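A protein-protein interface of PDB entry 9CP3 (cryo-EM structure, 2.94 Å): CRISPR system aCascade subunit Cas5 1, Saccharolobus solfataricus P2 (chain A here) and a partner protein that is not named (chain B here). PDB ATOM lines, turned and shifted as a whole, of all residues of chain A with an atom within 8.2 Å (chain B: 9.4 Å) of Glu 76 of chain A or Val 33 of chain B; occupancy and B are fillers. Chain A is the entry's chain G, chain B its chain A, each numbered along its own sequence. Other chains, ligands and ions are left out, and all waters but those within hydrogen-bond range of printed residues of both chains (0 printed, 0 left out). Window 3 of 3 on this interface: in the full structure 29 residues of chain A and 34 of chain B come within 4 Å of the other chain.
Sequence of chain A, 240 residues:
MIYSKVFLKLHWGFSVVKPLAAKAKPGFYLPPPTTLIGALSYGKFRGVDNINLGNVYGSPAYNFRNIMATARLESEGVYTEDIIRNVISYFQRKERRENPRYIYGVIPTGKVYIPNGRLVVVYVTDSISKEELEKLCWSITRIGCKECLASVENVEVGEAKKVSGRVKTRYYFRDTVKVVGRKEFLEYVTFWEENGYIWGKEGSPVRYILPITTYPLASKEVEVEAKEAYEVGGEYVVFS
Printed residues of chain B that touch a printed residue of chain A: Ala 30, Pro 31, Val 33 and Leu 146.
Hydrophobic or aromatic side chains of chain B that line the printed part of chain A: Ala 30, Pro 31, Val 33 and Leu 146.
Of the 19 printed residues of chain A, 4 touch a printed residue of chain B.
Hydrophobic or aromatic side chains of chain A within 4 Å of the printed part of chain B: Val 78, Tyr 113 and Pro 115.
Among the printed residues, 6 pairs touch across the chains.
Among the printed residues, no Asp or Glu carboxylate lies within 4 Å of a Lys or Arg side-chain nitrogen of the other chain.
Glu 74 of chain A touches none of the printed residues of chain B.
No residue of chain B comes within 4 Å of Ser 75 of chain A.
Glu 76 of chain A touches just one residue of chain B: Val 33 (3.9 Å).
Of the printed residues of chain B, Val 78 of chain A touches Pro 31 and Val 33.
Printed residues of chain B within 4 Å of Pro 115 of chain A: Leu 146 (3.7 Å).
Of the printed residues of chain A, Ala 30 of chain B touches Tyr 113 (3.5 Å).
Of the printed residues of chain A, Pro 31 of chain B touches Val 78 and Tyr 113.
Of chain A, only Glu 76 and Val 78 come within 4 Å of Val 33 of chain B.
The nearest residue of chain B that does not touch Glu 76 of chain A is Lys 35 of chain B (4.7 Å).
The nearest residue of chain A that does not touch Val 33 of chain B is Pro 216 of chain A (5.0 Å).
CG1 of Val 33 of chain B touches OE1 of Glu 76 of chain A, at 3.9 Å.
CB of Pro 31 of chain B touches CG1 of Val 78 of chain A (3.8 Å).
CG2 of Val 78 of chain A touches CG2 of Val 33 of chain B, 3.5 Å away.
CE2 of Tyr 113 of chain A touches CB of Ala 30 of chain B (3.5 Å).
Pro 31 of chain B touches Tyr 113 of chain A (O to CB, 3.8 Å).
Leu 146 of chain B touches Pro 115 of chain A (CD1 to CG, 3.7 Å).
The backbone NH (N) of Ala 30 of chain B lies within hydrogen-bond range of the backbone carbonyl oxygen (O) of Val 45 of chain B, 2.9 Å away.
The backbone carbonyl oxygen of Val 78 of chain A lies within hydrogen-bond range of the backbone NH of Tyr 113 of chain A (2.9 Å).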
ATOM      1  N   LEU A  73     -17.604  -0.438 -30.132  1.00  0.00           N
ATOM      2  CA  LEU A  73     -19.051  -0.464 -29.987  1.00  0.00           C
ATOM      3  C   LEU A  73     -19.672   0.784 -30.606  1.00  0.00           C
ATOM      4  O   LEU A  73     -19.013   1.809 -30.797  1.00  0.00           O
ATOM      5  CB  LEU A  73     -19.438  -0.590 -28.511  1.00  0.00           C
ATOM      6  CG  LEU A  73     -18.969   0.474 -27.512  1.00  0.00           C
ATOM      7  CD1 LEU A  73     -19.911   1.669 -27.455  1.00  0.00           C
ATOM      8  CD2 LEU A  73     -18.798  -0.140 -26.131  1.00  0.00           C
ATOM      9  N   GLU A  74     -20.965   0.685 -30.921  1.00  0.00           N
ATOM     10  CA  GLU A  74     -21.694   1.801 -31.509  1.00  0.00           C
ATOM     11  C   GLU A  74     -23.082   1.942 -30.889  1.00  0.00           C
ATOM     12  O   GLU A  74     -24.042   2.305 -31.577  1.00  0.00           O
ATOM     13  CB  GLU A  74     -21.790   1.643 -33.029  1.00  0.00           C
ATOM     14  CG  GLU A  74     -22.011   2.941 -33.792  1.00  0.00           C
ATOM     15  CD  GLU A  74     -21.965   2.746 -35.294  1.00  0.00           C
ATOM     16  OE1 GLU A  74     -21.760   1.598 -35.741  1.00  0.00           O
ATOM     17  OE2 GLU A  74     -22.135   3.742 -36.030  1.00  0.00           O
ATOM     18  N   SER A  75     -23.208   1.650 -29.598  1.00  0.00           N
ATOM     19  CA  SER A  75     -24.489   1.710 -28.900  1.00  0.00           C
ATOM     20  C   SER A  75     -24.211   1.883 -27.410  1.00  0.00           C
ATOM     21  O   SER A  75     -23.091   2.212 -27.004  1.00  0.00           O
ATOM     22  CB  SER A  75     -25.332   0.464 -29.188  1.00  0.00           C
ATOM     23  OG  SER A  75     -25.641   0.356 -30.566  1.00  0.00           O
ATOM     24  N   GLU A  76     -25.235   1.662 -26.592  1.00  0.00           N
ATOM     25  CA  GLU A  76     -25.134   1.790 -25.144  1.00  0.00           C
ATOM     26  C   GLU A  76     -25.301   0.420 -24.502  1.00  0.00           C
ATOM     27  O   GLU A  76     -26.228  -0.322 -24.844  1.00  0.00           O
ATOM     28  CB  GLU A  76     -26.191   2.759 -24.611  1.00  0.00           C
ATOM     29  CG  GLU A  76     -26.210   4.104 -25.319  1.00  0.00           C
ATOM     30  CD  GLU A  76     -27.480   4.888 -25.052  1.00  0.00           C
ATOM     31  OE1 GLU A  76     -28.466   4.283 -24.579  1.00  0.00           O
ATOM     32  OE2 GLU A  76     -27.493   6.109 -25.313  1.00  0.00           O
ATOM     33  N   GLY A  77     -24.406   0.092 -23.564  1.00  0.00           N
ATOM     34  CA  GLY A  77     -24.419  -1.207 -22.928  1.00  0.00           C
ATOM     35  C   GLY A  77     -24.218  -1.091 -21.430  1.00  0.00           C
ATOM     36  O   GLY A  77     -23.910  -0.020 -20.903  1.00  0.00           O
ATOM     37  N   VAL A  78     -24.399  -2.224 -20.752  1.00  0.00           N
ATOM     38  CA  VAL A  78     -24.338  -2.294 -19.297  1.00  0.00           C
ATOM     39  C   VAL A  78     -23.378  -3.409 -18.910  1.00  0.00           C
ATOM     40  O   VAL A  78     -23.205  -4.384 -19.645  1.00  0.00           O
ATOM     41  CB  VAL A  78     -25.737  -2.543 -18.680  1.00  0.00           C
ATOM     42  CG1 VAL A  78     -25.689  -2.515 -17.157  1.00  0.00           C
ATOM     43  CG2 VAL A  78     -26.741  -1.544 -19.205  1.00  0.00           C
ATOM     44  N   TYR A  79     -22.751  -3.263 -17.747  1.00  0.00           N
ATOM     45  CA  TYR A  79     -21.931  -4.313 -17.164  1.00  0.00           C
ATOM     46  C   TYR A  79     -22.680  -4.915 -15.985  1.00  0.00           C
ATOM     47  O   TYR A  79     -23.220  -4.182 -15.151  1.00  0.00           O
ATOM     48  CB  TYR A  79     -20.573  -3.774 -16.716  1.00  0.00           C
ATOM     49  CG  TYR A  79     -19.766  -4.766 -15.914  1.00  0.00           C
ATOM     50  CD1 TYR A  79     -19.153  -5.846 -16.531  1.00  0.00           C
ATOM     51  CD2 TYR A  79     -19.615  -4.623 -14.543  1.00  0.00           C
ATOM     52  CE1 TYR A  79     -18.413  -6.756 -15.809  1.00  0.00           C
ATOM     53  CE2 TYR A  79     -18.875  -5.529 -13.810  1.00  0.00           C
ATOM     54  CZ  TYR A  79     -18.277  -6.593 -14.448  1.00  0.00           C
ATOM     55  OH  TYR A  79     -17.540  -7.500 -13.723  1.00  0.00           O
ATOM     56  N   VAL A 112     -21.427  -8.444 -20.142  1.00  0.00           N
ATOM     57  CA  VAL A 112     -21.801  -7.178 -20.760  1.00  0.00           C
ATOM     58  C   VAL A 112     -23.081  -7.404 -21.550  1.00  0.00           C
ATOM     59  O   VAL A 112     -23.147  -8.309 -22.389  1.00  0.00           O
ATOM     60  CB  VAL A 112     -20.687  -6.630 -21.668  1.00  0.00           C
ATOM     61  CG1 VAL A 112     -21.201  -5.454 -22.481  1.00  0.00           C
ATOM     62  CG2 VAL A 112     -19.479  -6.226 -20.839  1.00  0.00           C
ATOM     63  N   TYR A 113     -24.089  -6.584 -21.282  1.00  0.00           N
ATOM     64  CA  TYR A 113     -25.369  -6.655 -21.969  1.00  0.00           C
ATOM     65  C   TYR A 113     -25.480  -5.489 -22.940  1.00  0.00           C
ATOM     66  O   TYR A 113     -25.400  -4.325 -22.530  1.00  0.00           O
ATOM     67  CB  TYR A 113     -26.527  -6.636 -20.973  1.00  0.00           C
ATOM     68  CG  TYR A 113     -26.849  -7.986 -20.381  1.00  0.00           C
ATOM     69  CD1 TYR A 113     -26.039  -8.548 -19.403  1.00  0.00           C
ATOM     70  CD2 TYR A 113     -27.964  -8.701 -20.798  1.00  0.00           C
ATOM     71  CE1 TYR A 113     -26.329  -9.782 -18.857  1.00  0.00           C
ATOM     72  CE2 TYR A 113     -28.262  -9.937 -20.259  1.00  0.00           C
ATOM     73  CZ  TYR A 113     -27.441 -10.471 -19.288  1.00  0.00           C
ATOM     74  OH  TYR A 113     -27.732 -11.702 -18.747  1.00  0.00           O
ATOM     75  N   ILE A 114     -25.652  -5.806 -24.218  1.00  0.00           N
ATOM     76  CA  ILE A 114     -25.927  -4.813 -25.254  1.00  0.00           C
ATOM     77  C   ILE A 114     -26.779  -5.501 -26.320  1.00  0.00           C
ATOM     78  O   ILE A 114     -26.333  -5.693 -27.461  1.00  0.00           O
ATOM     79  CB  ILE A 114     -24.620  -4.205 -25.802  1.00  0.00           C
ATOM     80  CG1 ILE A 114     -24.900  -3.149 -26.880  1.00  0.00           C
ATOM     81  CG2 ILE A 114     -23.631  -5.290 -26.251  1.00  0.00           C
ATOM     82  CD1 ILE A 114     -23.770  -2.166 -27.081  1.00  0.00           C
ATOM     83  N   PRO A 115     -28.004  -5.904 -25.991  1.00  0.00           N
ATOM     84  CA  PRO A 115     -28.822  -6.625 -26.969  1.00  0.00           C
ATOM     85  C   PRO A 115     -29.210  -5.737 -28.139  1.00  0.00           C
ATOM     86  O   PRO A 115     -29.399  -4.527 -27.997  1.00  0.00           O
ATOM     87  CB  PRO A 115     -30.052  -7.044 -26.159  1.00  0.00           C
ATOM     88  CG  PRO A 115     -30.135  -6.055 -25.066  1.00  0.00           C
ATOM     89  CD  PRO A 115     -28.729  -5.669 -24.731  1.00  0.00           C
ATOM     90  N   ASN A 116     -29.322  -6.364 -29.312  1.00  0.00           N
ATOM     91  CA  ASN A 116     -29.702  -5.700 -30.556  1.00  0.00           C
ATOM     92  C   ASN A 116     -28.751  -4.567 -30.928  1.00  0.00           C
ATOM     93  O   ASN A 116     -29.099  -3.701 -31.737  1.00  0.00           O
ATOM     94  CB  ASN A 116     -31.140  -5.175 -30.486  1.00  0.00           C
ATOM     95  CG  ASN A 116     -31.827  -5.184 -31.832  1.00  0.00           C
ATOM     96  OD1 ASN A 116     -31.473  -5.962 -32.717  1.00  0.00           O
ATOM     97  ND2 ASN A 116     -32.817  -4.317 -31.997  1.00  0.00           N
ATOM     98  N   GLY A 117     -27.549  -4.554 -30.356  1.00  0.00           N
ATOM     99  CA  GLY A 117     -26.601  -3.484 -30.577  1.00  0.00           C
ATOM    100  C   GLY A 117     -25.770  -3.683 -31.829  1.00  0.00           C
ATOM    101  O   GLY A 117     -26.025  -4.559 -32.658  1.00  0.00           O
ATOM    102  N   ARG A 118     -24.749  -2.841 -31.958  1.00  0.00           N
ATOM    103  CA  ARG A 118     -23.853  -2.853 -33.103  1.00  0.00           C
ATOM    104  C   ARG A 118     -22.411  -2.946 -32.631  1.00  0.00           C
ATOM    105  O   ARG A 118     -22.072  -2.555 -31.510  1.00  0.00           O
ATOM    106  CB  ARG A 118     -24.035  -1.597 -33.969  1.00  0.00           C
ATOM    107  CG  ARG A 118     -25.438  -1.408 -34.515  1.00  0.00           C
ATOM    108  CD  ARG A 118     -25.758  -2.437 -35.583  1.00  0.00           C
ATOM    109  NE  ARG A 118     -27.077  -2.224 -36.165  1.00  0.00           N
ATOM    110  CZ  ARG A 118     -27.295  -1.934 -37.441  1.00  0.00           C
ATOM    111  NH1 ARG A 118     -26.298  -1.810 -38.301  1.00  0.00           N
ATOM    112  NH2 ARG A 118     -28.545  -1.764 -37.863  1.00  0.00           N
ATOM    113  N   TYR A 215     -19.676   3.788 -16.548  1.00  0.00           N
ATOM    114  CA  TYR A 215     -21.096   3.563 -16.306  1.00  0.00           C
ATOM    115  C   TYR A 215     -21.925   4.759 -16.755  1.00  0.00           C
ATOM    116  O   TYR A 215     -21.813   5.845 -16.173  1.00  0.00           O
ATOM    117  CB  TYR A 215     -21.345   3.276 -14.825  1.00  0.00           C
ATOM    118  CG  TYR A 215     -22.795   3.021 -14.485  1.00  0.00           C
ATOM    119  CD1 TYR A 215     -23.537   2.080 -15.187  1.00  0.00           C
ATOM    120  CD2 TYR A 215     -23.422   3.718 -13.463  1.00  0.00           C
ATOM    121  CE1 TYR A 215     -24.863   1.842 -14.879  1.00  0.00           C
ATOM    122  CE2 TYR A 215     -24.747   3.486 -13.148  1.00  0.00           C
ATOM    123  CZ  TYR A 215     -25.463   2.548 -13.860  1.00  0.00           C
ATOM    124  OH  TYR A 215     -26.783   2.313 -13.551  1.00  0.00           O
ATOM    125  N   PRO A 216     -22.770   4.604 -17.781  1.00  0.00           N
ATOM    126  CA  PRO A 216     -22.968   3.403 -18.603  1.00  0.00           C
ATOM    127  C   PRO A 216     -21.841   3.232 -19.617  1.00  0.00           C
ATOM    128  O   PRO A 216     -21.114   4.180 -19.898  1.00  0.00           O
ATOM    129  CB  PRO A 216     -24.321   3.669 -19.270  1.00  0.00           C
ATOM    130  CG  PRO A 216     -24.368   5.160 -19.410  1.00  0.00           C
ATOM    131  CD  PRO A 216     -23.684   5.691 -18.173  1.00  0.00           C
ATOM    132  N   LEU A 217     -21.665   2.038 -20.174  1.00  0.00           N
ATOM    133  CA  LEU A 217     -20.568   1.803 -21.102  1.00  0.00           C
ATOM    134  C   LEU A 217     -20.822   2.503 -22.431  1.00  0.00           C
ATOM    135  O   LEU A 217     -21.917   2.416 -22.996  1.00  0.00           O
ATOM    136  CB  LEU A 217     -20.366   0.307 -21.325  1.00  0.00           C
ATOM    137  CG  LEU A 217     -19.775  -0.456 -20.142  1.00  0.00           C
ATOM    138  CD1 LEU A 217     -19.767  -1.944 -20.418  1.00  0.00           C
ATOM    139  CD2 LEU A 217     -18.370   0.038 -19.858  1.00  0.00           C
ATOM    140  N   ALA A 218     -19.800   3.196 -22.923  1.00  0.00           N
ATOM    141  CA  ALA A 218     -19.843   3.854 -24.221  1.00  0.00           C
ATOM    142  C   ALA A 218     -18.411   4.119 -24.656  1.00  0.00           C
ATOM    143  O   ALA A 218     -17.459   3.865 -23.916  1.00  0.00           O
ATOM    144  CB  ALA A 218     -20.657   5.150 -24.172  1.00  0.00           C
ATOM    145  N   SER A 219     -18.268   4.640 -25.870  1.00  0.00           N
ATOM    146  CA  SER A 219     -16.965   4.938 -26.443  1.00  0.00           C
ATOM    147  C   SER A 219     -16.831   6.439 -26.658  1.00  0.00           C
ATOM    148  O   SER A 219     -17.797   7.113 -27.027  1.00  0.00           O
ATOM    149  CB  SER A 219     -16.763   4.201 -27.767  1.00  0.00           C
ATOM    150  OG  SER A 219     -17.790   4.522 -28.688  1.00  0.00           O
ATOM    151  N   ALA B  30     -31.778  -9.141 -15.559  1.00  0.00           N
ATOM    152  CA  ALA B  30     -30.635  -8.507 -16.195  1.00  0.00           C
ATOM    153  C   ALA B  30     -30.916  -7.032 -16.450  1.00  0.00           C
ATOM    154  O   ALA B  30     -32.060  -6.654 -16.736  1.00  0.00           O
ATOM    155  CB  ALA B  30     -30.290  -9.202 -17.517  1.00  0.00           C
ATOM    156  N   PRO B  31     -29.900  -6.178 -16.328  1.00  0.00           N
ATOM    157  CA  PRO B  31     -30.094  -4.745 -16.586  1.00  0.00           C
ATOM    158  C   PRO B  31     -30.027  -4.412 -18.069  1.00  0.00           C
ATOM    159  O   PRO B  31     -29.181  -4.923 -18.806  1.00  0.00           O
ATOM    160  CB  PRO B  31     -28.925  -4.092 -15.837  1.00  0.00           C
ATOM    161  CG  PRO B  31     -28.474  -5.113 -14.846  1.00  0.00           C
ATOM    162  CD  PRO B  31     -28.696  -6.429 -15.522  1.00  0.00           C
ATOM    163  N   VAL B  32     -30.930  -3.531 -18.497  1.00  0.00           N
ATOM    164  CA  VAL B  32     -30.942  -3.001 -19.856  1.00  0.00           C
ATOM    165  C   VAL B  32     -31.256  -1.511 -19.794  1.00  0.00           C
ATOM    166  O   VAL B  32     -32.027  -1.052 -18.946  1.00  0.00           O
ATOM    167  CB  VAL B  32     -31.954  -3.732 -20.770  1.00  0.00           C
ATOM    168  CG1 VAL B  32     -31.558  -5.186 -20.964  1.00  0.00           C
ATOM    169  CG2 VAL B  32     -33.357  -3.639 -20.199  1.00  0.00           C
ATOM    170  N   VAL B  33     -30.647  -0.750 -20.700  1.00  0.00           N
ATOM    171  CA  VAL B  33     -30.868   0.690 -20.794  1.00  0.00           C
ATOM    172  C   VAL B  33     -31.807   0.977 -21.955  1.00  0.00           C
ATOM    173  O   VAL B  33     -31.567   0.536 -23.086  1.00  0.00           O
ATOM    174  CB  VAL B  33     -29.544   1.454 -20.960  1.00  0.00           C
ATOM    175  CG1 VAL B  33     -29.816   2.924 -21.183  1.00  0.00           C
ATOM    176  CG2 VAL B  33     -28.688   1.289 -19.726  1.00  0.00           C
ATOM    177  N   LEU B  34     -32.876   1.717 -21.675  1.00  0.00           N
ATOM    178  CA  LEU B  34     -33.841   2.146 -22.674  1.00  0.00           C
ATOM    179  C   LEU B  34     -33.658   3.637 -22.926  1.00  0.00           C
ATOM    180  O   LEU B  34     -33.542   4.423 -21.976  1.00  0.00           O
ATOM    181  CB  LEU B  34     -35.271   1.847 -22.217  1.00  0.00           C
ATOM    182  CG  LEU B  34     -36.381   1.988 -23.260  1.00  0.00           C
ATOM    183  CD1 LEU B  34     -37.363   0.836 -23.141  1.00  0.00           C
ATOM    184  CD2 LEU B  34     -37.099   3.321 -23.109  1.00  0.00           C
ATOM    185  N   LYS B  35     -33.624   4.017 -24.200  1.00  0.00           N
ATOM    186  CA  LYS B  35     -33.414   5.406 -24.580  1.00  0.00           C
ATOM    187  C   LYS B  35     -34.729   6.175 -24.533  1.00  0.00           C
ATOM    188  O   LYS B  35     -35.750   5.711 -25.050  1.00  0.00           O
ATOM    189  CB  LYS B  35     -32.806   5.488 -25.979  1.00  0.00           C
ATOM    190  CG  LYS B  35     -32.829   6.882 -26.582  1.00  0.00           C
ATOM    191  CD  LYS B  35     -32.002   6.953 -27.854  1.00  0.00           C
ATOM    192  CE  LYS B  35     -32.195   8.283 -28.562  1.00  0.00           C
ATOM    193  NZ  LYS B  35     -33.577   8.429 -29.098  1.00  0.00           N
ATOM    194  N   THR B  36     -34.700   7.351 -23.911  1.00  0.00           N
ATOM    195  CA  THR B  36     -35.854   8.232 -23.819  1.00  0.00           C
ATOM    196  C   THR B  36     -35.447   9.635 -24.247  1.00  0.00           C
ATOM    197  O   THR B  36     -34.261   9.955 -24.365  1.00  0.00           O
ATOM    198  CB  THR B  36     -36.439   8.261 -22.399  1.00  0.00           C
ATOM    199  OG1 THR B  36     -35.441   8.716 -21.476  1.00  0.00           O
ATOM    200  CG2 THR B  36     -36.919   6.879 -21.986  1.00  0.00           C
ATOM    201  N   GLY B  39     -33.626  11.250 -21.368  1.00  0.00           N
ATOM    202  CA  GLY B  39     -32.331  10.631 -21.168  1.00  0.00           C
ATOM    203  C   GLY B  39     -32.374   9.124 -21.312  1.00  0.00           C
ATOM    204  O   GLY B  39     -32.984   8.599 -22.248  1.00  0.00           O
ATOM    205  N   TYR B  40     -31.726   8.416 -20.392  1.00  0.00           N
ATOM    206  CA  TYR B  40     -31.691   6.963 -20.402  1.00  0.00           C
ATOM    207  C   TYR B  40     -32.311   6.424 -19.121  1.00  0.00           C
ATOM    208  O   TYR B  40     -32.209   7.042 -18.057  1.00  0.00           O
ATOM    209  CB  TYR B  40     -30.253   6.447 -20.554  1.00  0.00           C
ATOM    210  CG  TYR B  40     -29.277   7.012 -19.543  1.00  0.00           C
ATOM    211  CD1 TYR B  40     -29.160   6.461 -18.274  1.00  0.00           C
ATOM    212  CD2 TYR B  40     -28.473   8.098 -19.860  1.00  0.00           C
ATOM    213  CE1 TYR B  40     -28.270   6.974 -17.350  1.00  0.00           C
ATOM    214  CE2 TYR B  40     -27.580   8.619 -18.942  1.00  0.00           C
ATOM    215  CZ  TYR B  40     -27.483   8.053 -17.689  1.00  0.00           C
ATOM    216  OH  TYR B  40     -26.597   8.567 -16.772  1.00  0.00           O
ATOM    217  N   LEU B  41     -32.963   5.269 -19.228  1.00  0.00           N
ATOM    218  CA  LEU B  41     -33.577   4.608 -18.083  1.00  0.00           C
ATOM    219  C   LEU B  41     -33.011   3.202 -17.952  1.00  0.00           C
ATOM    220  O   LEU B  41     -33.091   2.408 -18.893  1.00  0.00           O
ATOM    221  CB  LEU B  41     -35.100   4.557 -18.226  1.00  0.00           C
ATOM    222  CG  LEU B  41     -35.816   5.893 -18.410  1.00  0.00           C
ATOM    223  CD1 LEU B  41     -37.317   5.680 -18.510  1.00  0.00           C
ATOM    224  CD2 LEU B  41     -35.480   6.839 -17.270  1.00  0.00           C
ATOM    225  N   VAL B  42     -32.448   2.895 -16.790  1.00  0.00           N
ATOM    226  CA  VAL B  42     -31.947   1.556 -16.506  1.00  0.00           C
ATOM    227  C   VAL B  42     -33.073   0.742 -15.880  1.00  0.00           C
ATOM    228  O   VAL B  42     -33.753   1.201 -14.953  1.00  0.00           O
ATOM    229  CB  VAL B  42     -30.702   1.609 -15.600  1.00  0.00           C
ATOM    230  CG1 VAL B  42     -31.026   2.196 -14.232  1.00  0.00           C
ATOM    231  CG2 VAL B  42     -30.094   0.223 -15.456  1.00  0.00           C
ATOM    232  N   ARG B  43     -33.305  -0.453 -16.416  1.00  0.00           N
ATOM    233  CA  ARG B  43     -34.393  -1.309 -15.976  1.00  0.00           C
ATOM    234  C   ARG B  43     -33.879  -2.730 -15.810  1.00  0.00           C
ATOM    235  O   ARG B  43     -32.853  -3.113 -16.378  1.00  0.00           O
ATOM    236  CB  ARG B  43     -35.557  -1.308 -16.976  1.00  0.00           C
ATOM    237  CG  ARG B  43     -36.213   0.037 -17.201  1.00  0.00           C
ATOM    238  CD  ARG B  43     -37.060   0.451 -16.015  1.00  0.00           C
ATOM    239  NE  ARG B  43     -37.720   1.728 -16.252  1.00  0.00           N
ATOM    240  CZ  ARG B  43     -38.881   1.866 -16.877  1.00  0.00           C
ATOM    241  NH1 ARG B  43     -39.540   0.820 -17.349  1.00  0.00           N
ATOM    242  NH2 ARG B  43     -39.391   3.084 -17.039  1.00  0.00           N
ATOM    243  N   TYR B  44     -34.606  -3.511 -15.020  1.00  0.00           N
ATOM    244  CA  TYR B  44     -34.277  -4.906 -14.774  1.00  0.00           C
ATOM    245  C   TYR B  44     -35.354  -5.774 -15.402  1.00  0.00           C
ATOM    246  O   TYR B  44     -36.545  -5.584 -15.136  1.00  0.00           O
ATOM    247  CB  TYR B  44     -34.155  -5.197 -13.277  1.00  0.00           C
ATOM    248  CG  TYR B  44     -32.920  -4.607 -12.637  1.00  0.00           C
ATOM    249  CD1 TYR B  44     -32.729  -3.234 -12.578  1.00  0.00           C
ATOM    250  CD2 TYR B  44     -31.937  -5.428 -12.100  1.00  0.00           C
ATOM    251  CE1 TYR B  44     -31.599  -2.696 -11.997  1.00  0.00           C
ATOM    252  CE2 TYR B  44     -30.804  -4.899 -11.517  1.00  0.00           C
ATOM    253  CZ  TYR B  44     -30.640  -3.532 -11.469  1.00  0.00           C
ATOM    254  OH  TYR B  44     -29.513  -2.998 -10.889  1.00  0.00           O
ATOM    255  N   VAL B  45     -34.938  -6.722 -16.235  1.00  0.00           N
ATOM    256  CA  VAL B  45     -35.891  -7.543 -16.976  1.00  0.00           C
ATOM    257  C   VAL B  45     -35.632  -9.013 -16.667  1.00  0.00           C
ATOM    258  O   VAL B  45     -34.471  -9.422 -16.536  1.00  0.00           O
ATOM    259  CB  VAL B  45     -35.808  -7.261 -18.484  1.00  0.00           C
ATOM    260  CG1 VAL B  45     -36.225  -5.833 -18.772  1.00  0.00           C
ATOM    261  CG2 VAL B  45     -34.400  -7.507 -18.996  1.00  0.00           C
ATOM    262  N   LEU B 146     -36.213  -6.245 -26.787  1.00  0.00           N
ATOM    263  CA  LEU B 146     -36.214  -4.791 -26.653  1.00  0.00           C
ATOM    264  C   LEU B 146     -36.746  -4.202 -27.952  1.00  0.00           C
ATOM    265  O   LEU B 146     -35.997  -3.913 -28.885  1.00  0.00           O
ATOM    266  CB  LEU B 146     -34.817  -4.273 -26.332  1.00  0.00           C
ATOM    267  CG  LEU B 146     -34.144  -4.800 -25.066  1.00  0.00           C
ATOM    268  CD1 LEU B 146     -33.026  -3.865 -24.644  1.00  0.00           C
ATOM    269  CD2 LEU B 146     -35.152  -4.965 -23.940  1.00  0.00           C
ATOM    270  N   ARG B 147     -38.061  -4.024 -28.011  1.00  0.00           N
ATOM    271  CA  ARG B 147     -38.737  -3.538 -29.204  1.00  0.00           C
ATOM    272  C   ARG B 147     -39.465  -2.243 -28.879  1.00  0.00           C
ATOM    273  O   ARG B 147     -40.126  -2.137 -27.841  1.00  0.00           O
ATOM    274  CB  ARG B 147     -39.732  -4.576 -29.730  1.00  0.00           C
ATOM    275  CG  ARG B 147     -40.718  -4.035 -30.745  1.00  0.00           C
ATOM    276  CD  ARG B 147     -41.741  -5.087 -31.126  1.00  0.00           C
ATOM    277  NE  ARG B 147     -42.729  -5.261 -30.069  1.00  0.00           N
ATOM    278  CZ  ARG B 147     -43.773  -4.465 -29.886  1.00  0.00           C
ATOM    279  NH1 ARG B 147     -44.010  -3.439 -30.686  1.00  0.00           N
ATOM    280  NH2 ARG B 147     -44.598  -4.700 -28.870  1.00  0.00           N
ATOM    281  N   GLY B 148     -39.344  -1.262 -29.769  1.00  0.00           N
ATOM    282  CA  GLY B 148     -39.984   0.020 -29.523  1.00  0.00           C
ATOM    283  C   GLY B 148     -39.342   0.746 -28.356  1.00  0.00           C
ATOM    284  O   GLY B 148     -38.127   0.682 -28.140  1.00  0.00           O
ATOM    285  N   ASP B 149     -40.173   1.447 -27.586  1.00  0.00           N
ATOM    286  CA  ASP B 149     -39.719   2.212 -26.432  1.00  0.00           C
ATOM    287  C   ASP B 149     -40.239   1.647 -25.115  1.00  0.00           C
ATOM    288  O   ASP B 149     -40.159   2.325 -24.087  1.00  0.00           O
ATOM    289  CB  ASP B 149     -40.132   3.677 -26.574  1.00  0.00           C
ATOM    290  CG  ASP B 149     -39.330   4.407 -27.634  1.00  0.00           C
ATOM    291  OD1 ASP B 149     -38.499   3.759 -28.304  1.00  0.00           O
ATOM    292  OD2 ASP B 149     -39.528   5.630 -27.796  1.00  0.00           O
ATOM    293  N   ILE B 151     -40.715  -2.166 -22.644  1.00  0.00           N
ATOM    294  CA  ILE B 151     -40.321  -3.548 -22.395  1.00  0.00           C
ATOM    295  C   ILE B 151     -41.542  -4.302 -21.882  1.00  0.00           C
ATOM    296  O   ILE B 151     -42.041  -3.988 -20.793  1.00  0.00           O
ATOM    297  CB  ILE B 151     -39.161  -3.637 -21.393  1.00  0.00           C
ATOM    298  CG1 ILE B 151     -38.048  -2.663 -21.782  1.00  0.00           C
ATOM    299  CG2 ILE B 151     -38.632  -5.057 -21.331  1.00  0.00           C
ATOM    300  CD1 ILE B 151     -36.820  -2.765 -20.911  1.00  0.00           C
